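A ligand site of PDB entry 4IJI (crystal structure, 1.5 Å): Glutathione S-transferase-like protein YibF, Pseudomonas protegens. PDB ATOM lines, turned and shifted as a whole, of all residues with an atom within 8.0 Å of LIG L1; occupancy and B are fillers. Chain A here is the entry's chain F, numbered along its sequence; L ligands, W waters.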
ATOM      1  N   ASN A   8      18.750   6.342 -10.338  1.00  0.00           N
ATOM      2  CA  ASN A   8      19.473   7.249  -9.464  1.00  0.00           C
ATOM      3  C   ASN A   8      19.684   8.537 -10.242  1.00  0.00           C
ATOM      4  O   ASN A   8      20.045   8.492 -11.427  1.00  0.00           O
ATOM      5  CB  ASN A   8      20.811   6.659  -9.042  1.00  0.00           C
ATOM      6  CG  ASN A   8      21.703   7.673  -8.373  1.00  0.00           C
ATOM      7  OD1 ASN A   8      22.441   8.401  -9.039  1.00  0.00           O
ATOM      8  ND2 ASN A   8      21.619   7.747  -7.052  1.00  0.00           N
ATOM      9  N   PRO A   9      19.449   9.698  -9.625  1.00  0.00           N
ATOM     10  CA  PRO A   9      19.455  10.937 -10.394  1.00  0.00           C
ATOM     11  C   PRO A   9      20.847  11.537 -10.631  1.00  0.00           C
ATOM     12  O   PRO A   9      20.931  12.527 -11.360  1.00  0.00           O
ATOM     13  CB  PRO A   9      18.613  11.881  -9.537  1.00  0.00           C
ATOM     14  CG  PRO A   9      18.867  11.412  -8.148  1.00  0.00           C
ATOM     15  CD  PRO A   9      19.040   9.917  -8.225  1.00  0.00           C
ATOM     16  N   ALA A  10      21.882  10.966 -10.031  1.00  0.00           N
ATOM     17  CA  ALA A  10      23.253  11.434 -10.233  1.00  0.00           C
ATOM     18  C   ALA A  10      23.985  10.645 -11.320  1.00  0.00           C
ATOM     19  O   ALA A  10      24.932  11.148 -11.941  1.00  0.00           O
ATOM     20  CB  ALA A  10      24.035  11.348  -8.925  1.00  0.00           C
ATOM     21  N   SER A  11      23.572   9.408 -11.550  1.00  0.00           N
ATOM     22  CA  SER A  11      24.298   8.542 -12.475  1.00  0.00           C
ATOM     23  C   SER A  11      24.211   9.020 -13.917  1.00  0.00           C
ATOM     24  O   SER A  11      23.125   9.259 -14.443  1.00  0.00           O
ATOM     25  CB  SER A  11      23.759   7.128 -12.394  1.00  0.00           C
ATOM     26  OG  SER A  11      24.265   6.370 -13.469  1.00  0.00           O
ATOM     27  N   PRO A  12      25.375   9.149 -14.592  1.00  0.00           N
ATOM     28  CA  PRO A  12      25.334   9.568 -15.994  1.00  0.00           C
ATOM     29  C   PRO A  12      24.872   8.440 -16.899  1.00  0.00           C
ATOM     30  O   PRO A  12      24.402   8.720 -18.001  1.00  0.00           O
ATOM     31  CB  PRO A  12      26.786   9.931 -16.277  1.00  0.00           C
ATOM     32  CG  PRO A  12      27.586   9.046 -15.350  1.00  0.00           C
ATOM     33  CD  PRO A  12      26.743   8.930 -14.092  1.00  0.00           C
ATOM     34  N   TYR A  13      24.973   7.196 -16.430  1.00  0.00           N
ATOM     35  CA  TYR A  13      24.506   6.042 -17.181  1.00  0.00           C
ATOM     36  C   TYR A  13      22.979   5.986 -17.147  1.00  0.00           C
ATOM     37  O   TYR A  13      22.334   5.760 -18.174  1.00  0.00           O
ATOM     38  CB  TYR A  13      25.102   4.752 -16.617  1.00  0.00           C
ATOM     39  CG  TYR A  13      26.624   4.773 -16.521  1.00  0.00           C
ATOM     40  CD1 TYR A  13      27.423   4.489 -17.628  1.00  0.00           C
ATOM     41  CD2 TYR A  13      27.249   5.053 -15.325  1.00  0.00           C
ATOM     42  CE1 TYR A  13      28.798   4.503 -17.529  1.00  0.00           C
ATOM     43  CE2 TYR A  13      28.618   5.062 -15.215  1.00  0.00           C
ATOM     44  CZ  TYR A  13      29.388   4.788 -16.315  1.00  0.00           C
ATOM     45  OH  TYR A  13      30.753   4.807 -16.148  1.00  0.00           O
ATOM     46  N   VAL A  14      22.400   6.202 -15.969  1.00  0.00           N
ATOM     47  CA  VAL A  14      20.961   6.432 -15.877  1.00  0.00           C
ATOM     48  C   VAL A  14      20.510   7.613 -16.730  1.00  0.00           C
ATOM     49  O   VAL A  14      19.479   7.546 -17.402  1.00  0.00           O
ATOM     50  CB  VAL A  14      20.510   6.658 -14.408  1.00  0.00           C
ATOM     51  CG1 VAL A  14      19.040   7.038 -14.372  1.00  0.00           C
ATOM     52  CG2 VAL A  14      20.749   5.414 -13.558  1.00  0.00           C
ATOM     53  N   LEU A  37      22.859   3.346  -4.259  1.00  0.00           N
ATOM     54  CA  LEU A  37      24.212   3.139  -4.744  1.00  0.00           C
ATOM     55  C   LEU A  37      25.007   2.375  -3.702  1.00  0.00           C
ATOM     56  O   LEU A  37      24.764   2.501  -2.506  1.00  0.00           O
ATOM     57  CB  LEU A  37      24.888   4.477  -5.045  1.00  0.00           C
ATOM     58  CG  LEU A  37      24.122   5.384  -6.022  1.00  0.00           C
ATOM     59  CD1 LEU A  37      24.794   6.754  -6.139  1.00  0.00           C
ATOM     60  CD2 LEU A  37      24.006   4.716  -7.383  1.00  0.00           C
ATOM     61  N   SER A  38      25.955   1.562  -4.162  1.00  0.00           N
ATOM     62  CA  SER A  38      26.852   0.830  -3.260  1.00  0.00           C
ATOM     63  C   SER A  38      28.263   0.790  -3.831  1.00  0.00           C
ATOM     64  O   SER A  38      28.804  -0.290  -4.089  1.00  0.00           O
ATOM     65  CB  SER A  38      26.333  -0.592  -3.030  1.00  0.00           C
ATOM     66  OG  SER A  38      26.338  -1.336  -4.246  1.00  0.00           O
ATOM     67  N   PRO A  39      28.883   1.963  -4.000  1.00  0.00           N
ATOM     68  CA  PRO A  39      30.148   2.042  -4.751  1.00  0.00           C
ATOM     69  C   PRO A  39      31.340   1.421  -4.009  1.00  0.00           C
ATOM     70  O   PRO A  39      32.328   1.042  -4.656  1.00  0.00           O
ATOM     71  CB  PRO A  39      30.348   3.550  -4.921  1.00  0.00           C
ATOM     72  CG  PRO A  39      29.671   4.141  -3.719  1.00  0.00           C
ATOM     73  CD  PRO A  39      28.494   3.266  -3.432  1.00  0.00           C
ATOM     74  N   ILE A  55      22.206  -0.495 -11.769  1.00  0.00           N
ATOM     75  CA  ILE A  55      21.598   0.837 -11.970  1.00  0.00           C
ATOM     76  C   ILE A  55      22.274   1.521 -13.167  1.00  0.00           C
ATOM     77  O   ILE A  55      23.477   1.776 -13.156  1.00  0.00           O
ATOM     78  CB  ILE A  55      21.733   1.725 -10.715  1.00  0.00           C
ATOM     79  CG1 ILE A  55      21.091   1.082  -9.487  1.00  0.00           C
ATOM     80  CG2 ILE A  55      21.096   3.079 -10.957  1.00  0.00           C
ATOM     81  CD1 ILE A  55      21.454   1.786  -8.182  1.00  0.00           C
ATOM     82  N   PRO A  56      21.509   1.818 -14.230  1.00  0.00           N
ATOM     83  CA  PRO A  56      20.081   1.542 -14.389  1.00  0.00           C
ATOM     84  C   PRO A  56      19.805   0.056 -14.617  1.00  0.00           C
ATOM     85  O   PRO A  56      20.663  -0.703 -15.046  1.00  0.00           O
ATOM     86  CB  PRO A  56      19.728   2.305 -15.672  1.00  0.00           C
ATOM     87  CG  PRO A  56      21.025   2.322 -16.455  1.00  0.00           C
ATOM     88  CD  PRO A  56      22.103   2.425 -15.434  1.00  0.00           C
ATOM     89  N   MET A 107      32.855   8.474 -19.227  1.00  0.00           N
ATOM     90  CA  MET A 107      32.148   8.252 -17.967  1.00  0.00           C
ATOM     91  C   MET A 107      32.882   7.295 -17.061  1.00  0.00           C
ATOM     92  O   MET A 107      33.045   7.593 -15.867  1.00  0.00           O
ATOM     93  CB  MET A 107      30.727   7.743 -18.207  1.00  0.00           C
ATOM     94  CG  MET A 107      29.816   8.763 -18.833  1.00  0.00           C
ATOM     95  SD  MET A 107      28.050   7.971 -19.166  1.00  0.00           S
ATOM     96  CE  MET A 107      27.291   9.428 -20.093  1.00  0.00           C
ATOM     97  N   SER A 110      35.847   8.997 -15.564  1.00  0.00           N
ATOM     98  CA  SER A 110      35.345  10.050 -14.691  1.00  0.00           C
ATOM     99  C   SER A 110      34.844   9.468 -13.377  1.00  0.00           C
ATOM    100  O   SER A 110      35.075  10.038 -12.297  1.00  0.00           O
ATOM    101  CB  SER A 110      34.225  10.824 -15.375  1.00  0.00           C
ATOM    102  OG  SER A 110      34.693  11.459 -16.546  1.00  0.00           O
ATOM    103  N   VAL A 111      34.126   8.348 -13.459  1.00  0.00           N
ATOM    104  CA  VAL A 111      33.616   7.712 -12.259  1.00  0.00           C
ATOM    105  C   VAL A 111      34.765   7.172 -11.400  1.00  0.00           C
ATOM    106  O   VAL A 111      34.754   7.333 -10.179  1.00  0.00           O
ATOM    107  CB  VAL A 111      32.614   6.621 -12.593  1.00  0.00           C
ATOM    108  CG1 VAL A 111      32.297   5.810 -11.349  1.00  0.00           C
ATOM    109  CG2 VAL A 111      31.342   7.245 -13.183  1.00  0.00           C
ATOM    110  N   LEU A 112      35.753   6.553 -12.030  1.00  0.00           N
ATOM    111  CA  LEU A 112      36.909   6.027 -11.294  1.00  0.00           C
ATOM    112  C   LEU A 112      37.625   7.133 -10.551  1.00  0.00           C
ATOM    113  O   LEU A 112      37.964   6.971  -9.382  1.00  0.00           O
ATOM    114  CB  LEU A 112      37.882   5.286 -12.210  1.00  0.00           C
ATOM    115  CG  LEU A 112      37.440   3.916 -12.704  1.00  0.00           C
ATOM    116  CD1 LEU A 112      38.563   3.313 -13.562  1.00  0.00           C
ATOM    117  CD2 LEU A 112      37.117   2.987 -11.551  1.00  0.00           C
ATOM    118  N   ARG A 114      36.311  10.043  -9.657  1.00  0.00           N
ATOM    119  CA  ARG A 114      35.375  10.452  -8.608  1.00  0.00           C
ATOM    120  C   ARG A 114      35.406   9.526  -7.405  1.00  0.00           C
ATOM    121  O   ARG A 114      35.517   9.983  -6.264  1.00  0.00           O
ATOM    122  CB  ARG A 114      33.955  10.544  -9.176  1.00  0.00           C
ATOM    123  CG  ARG A 114      32.864  10.692  -8.118  1.00  0.00           C
ATOM    124  CD  ARG A 114      32.996  11.994  -7.371  1.00  0.00           C
ATOM    125  NE  ARG A 114      32.034  12.074  -6.268  1.00  0.00           N
ATOM    126  CZ  ARG A 114      31.870  13.150  -5.512  1.00  0.00           C
ATOM    127  NH1 ARG A 114      32.603  14.224  -5.723  1.00  0.00           N
ATOM    128  NH2 ARG A 114      30.977  13.140  -4.515  1.00  0.00           N
ATOM    129  N   TYR A 115      35.288   8.222  -7.636  1.00  0.00           N
ATOM    130  CA  TYR A 115      35.217   7.280  -6.517  1.00  0.00           C
ATOM    131  C   TYR A 115      36.492   7.294  -5.707  1.00  0.00           C
ATOM    132  O   TYR A 115      36.462   7.208  -4.484  1.00  0.00           O
ATOM    133  CB  TYR A 115      34.934   5.852  -6.995  1.00  0.00           C
ATOM    134  CG  TYR A 115      33.503   5.591  -7.406  1.00  0.00           C
ATOM    135  CD1 TYR A 115      32.514   6.556  -7.221  1.00  0.00           C
ATOM    136  CD2 TYR A 115      33.143   4.386  -7.981  1.00  0.00           C
ATOM    137  CE1 TYR A 115      31.208   6.320  -7.592  1.00  0.00           C
ATOM    138  CE2 TYR A 115      31.838   4.134  -8.369  1.00  0.00           C
ATOM    139  CZ  TYR A 115      30.879   5.097  -8.167  1.00  0.00           C
ATOM    140  OH  TYR A 115      29.586   4.838  -8.553  1.00  0.00           O
ATOM    141  N   ALA A 118      36.499  10.851  -3.790  1.00  0.00           N
ATOM    142  CA  ALA A 118      35.367  11.059  -2.894  1.00  0.00           C
ATOM    143  C   ALA A 118      35.229   9.956  -1.844  1.00  0.00           C
ATOM    144  O   ALA A 118      34.632  10.188  -0.793  1.00  0.00           O
ATOM    145  CB  ALA A 118      34.071  11.160  -3.709  1.00  0.00           C
ATOM    146  N   TYR A 169      28.491  15.108 -16.711  1.00  0.00           N
ATOM    147  CA  TYR A 169      29.090  14.469 -15.555  1.00  0.00           C
ATOM    148  C   TYR A 169      30.436  15.099 -15.204  1.00  0.00           C
ATOM    149  O   TYR A 169      30.793  15.220 -14.029  1.00  0.00           O
ATOM    150  CB  TYR A 169      29.224  12.956 -15.770  1.00  0.00           C
ATOM    151  CG  TYR A 169      29.627  12.244 -14.513  1.00  0.00           C
ATOM    152  CD1 TYR A 169      28.711  12.038 -13.488  1.00  0.00           C
ATOM    153  CD2 TYR A 169      30.924  11.801 -14.341  1.00  0.00           C
ATOM    154  CE1 TYR A 169      29.085  11.394 -12.327  1.00  0.00           C
ATOM    155  CE2 TYR A 169      31.307  11.156 -13.184  1.00  0.00           C
ATOM    156  CZ  TYR A 169      30.387  10.949 -12.189  1.00  0.00           C
ATOM    157  OH  TYR A 169      30.800  10.308 -11.041  1.00  0.00           O
ATOM    158  N   PHE A 172      29.742  18.245 -13.381  1.00  0.00           N
ATOM    159  CA  PHE A 172      29.175  17.898 -12.081  1.00  0.00           C
ATOM    160  C   PHE A 172      30.232  17.454 -11.072  1.00  0.00           C
ATOM    161  O   PHE A 172      30.292  17.978  -9.960  1.00  0.00           O
ATOM    162  CB  PHE A 172      28.147  16.772 -12.323  1.00  0.00           C
ATOM    163  CG  PHE A 172      27.506  16.222 -11.072  1.00  0.00           C
ATOM    164  CD1 PHE A 172      27.027  17.059 -10.075  1.00  0.00           C
ATOM    165  CD2 PHE A 172      27.340  14.852 -10.936  1.00  0.00           C
ATOM    166  CE1 PHE A 172      26.412  16.530  -8.932  1.00  0.00           C
ATOM    167  CE2 PHE A 172      26.732  14.313  -9.821  1.00  0.00           C
ATOM    168  CZ  PHE A 172      26.269  15.148  -8.816  1.00  0.00           C
ATOM    169  N   ARG A 173      31.053  16.474 -11.449  1.00  0.00           N
ATOM    170  CA  ARG A 173      31.982  15.883 -10.501  1.00  0.00           C
ATOM    171  C   ARG A 173      33.397  16.408 -10.630  1.00  0.00           C
ATOM    172  O   ARG A 173      34.162  16.354  -9.672  1.00  0.00           O
ATOM    173  CB  ARG A 173      32.013  14.356 -10.648  1.00  0.00           C
ATOM    174  CG  ARG A 173      30.757  13.656 -10.162  1.00  0.00           C
ATOM    175  CD  ARG A 173      30.336  14.180  -8.797  1.00  0.00           C
ATOM    176  NE  ARG A 173      29.382  13.295  -8.139  1.00  0.00           N
ATOM    177  CZ  ARG A 173      28.727  13.622  -7.027  1.00  0.00           C
ATOM    178  NH1 ARG A 173      28.926  14.807  -6.473  1.00  0.00           N
ATOM    179  NH2 ARG A 173      27.865  12.765  -6.480  1.00  0.00           N
ATOM    180  N   HIS A 174      33.754  16.912 -11.807  1.00  0.00           N
ATOM    181  CA  HIS A 174      35.131  17.351 -12.012  1.00  0.00           C
ATOM    182  C   HIS A 174      35.223  18.762 -12.588  1.00  0.00           C
ATOM    183  O   HIS A 174      35.824  18.949 -13.650  1.00  0.00           O
ATOM    184  CB  HIS A 174      35.857  16.366 -12.929  1.00  0.00           C
ATOM    185  CG  HIS A 174      35.813  14.952 -12.434  1.00  0.00           C
ATOM    186  ND1 HIS A 174      36.411  14.565 -11.254  1.00  0.00           N
ATOM    187  CD2 HIS A 174      35.213  13.840 -12.926  1.00  0.00           C
ATOM    188  CE1 HIS A 174      36.198  13.266 -11.054  1.00  0.00           C
ATOM    189  NE2 HIS A 174      35.475  12.815 -12.065  1.00  0.00           N
ATOM    190  N   PRO A 204      22.030  16.448 -12.839  1.00  0.00           N
ATOM    191  CA  PRO A 204      22.310  15.793 -11.550  1.00  0.00           C
ATOM    192  C   PRO A 204      22.087  16.763 -10.374  1.00  0.00           C
ATOM    193  O   PRO A 204      22.274  17.974 -10.537  1.00  0.00           O
ATOM    194  CB  PRO A 204      23.794  15.401 -11.665  1.00  0.00           C
ATOM    195  CG  PRO A 204      24.372  16.363 -12.638  1.00  0.00           C
ATOM    196  CD  PRO A 204      23.259  16.621 -13.642  1.00  0.00           C
ATOM    197  N   PRO A 205      21.661  16.244  -9.218  1.00  0.00           N
ATOM    198  CA  PRO A 205      21.326  17.109  -8.080  1.00  0.00           C
ATOM    199  C   PRO A 205      22.526  17.825  -7.464  1.00  0.00           C
ATOM    200  O   PRO A 205      23.618  17.255  -7.394  1.00  0.00           O
ATOM    201  CB  PRO A 205      20.697  16.132  -7.072  1.00  0.00           C
ATOM    202  CG  PRO A 205      21.228  14.783  -7.459  1.00  0.00           C
ATOM    203  CD  PRO A 205      21.391  14.813  -8.941  1.00  0.00           C
HETATM  204  C1  LIG L   1      28.088   9.922  -8.707  1.00  0.00           C
HETATM  205  O1  LIG L   1      27.460  10.410  -7.736  1.00  0.00           O
HETATM  206  O2  LIG L   1      29.109  10.501  -9.112  1.00  0.00           O
HETATM  207  C2  LIG L   1      27.626   8.666  -9.357  1.00  0.00           C
HETATM  208  C3  LIG L   1      26.367   8.141  -9.077  1.00  0.00           C
HETATM  209  C4  LIG L   1      25.958   6.967  -9.690  1.00  0.00           C
HETATM  210  C5  LIG L   1      26.785   6.320 -10.604  1.00  0.00           C
HETATM  211  C6  LIG L   1      28.042   6.853 -10.891  1.00  0.00           C
HETATM  212  C7  LIG L   1      28.454   8.019 -10.271  1.00  0.00           C
HETATM  213  C1  LG2 L   2      26.937   0.749 -16.234  1.00  0.00           C
HETATM  214  C2  LG2 L   2      28.040   1.537 -16.046  1.00  0.00           C
HETATM  215  C3  LG2 L   2      25.908   1.083 -17.249  1.00  0.00           C
HETATM  216  O1  LG2 L   2      26.241   1.543 -18.373  1.00  0.00           O
HETATM  217  O2  LG2 L   2      24.690   0.880 -16.991  1.00  0.00           O
HETATM  218  O   HOH W   1      25.595  10.442  -5.686  1.00  0.00           O
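The side-chain amide oxygen (OD1) of Asn 8 sits at hydrogen-bond distance from the backbone NH (N) of Ser 11 (2.9 Å). The backbone NH (N) of Ala 10 is in hydrogen-bond range of the side-chain amide oxygen (OD1) of Asn 8 (2.8 Å). The backbone NH (N) of Val 14 sits at hydrogen-bond distance from the side-chain hydroxyl (OG) of Ser 11 (3.1 Å). The side-chain hydroxyl (OG) of Ser 11 lies within hydrogen-bond range of the backbone NH (N) of Tyr 13, 3.2 Å away.
Residues that only touch LIG L1: Tyr 115 (3.5 Å), Ser 11 (3.5 Å), Leu 37 (3.6 Å), Ala 10 (3.7 Å), Asn 8 (3.9 Å) and Arg 114 (3.9 Å). Eight residues have an atom within 4 Å of LIG L1: Asn 8, Ala 10, Ser 11, Leu 37, Arg 114, Tyr 115, Tyr 169 and Arg 173. The nearest printed residue that does not touch LIG L1 is Pro 12 (4.03 Å).
Water W1 lies within hydrogen-bond range of an oxygen (O1) of LIG L1 (2.8 Å) and the guanidinium group of Arg 173 (3.3 Å).
NH2 of Arg 173 lies within salt-bridge range of O1 of LIG L1 (2.7 Å). OH of Tyr 169 sits at hydrogen-bond distance from O2 of LIG L1, at 2.6 Å.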
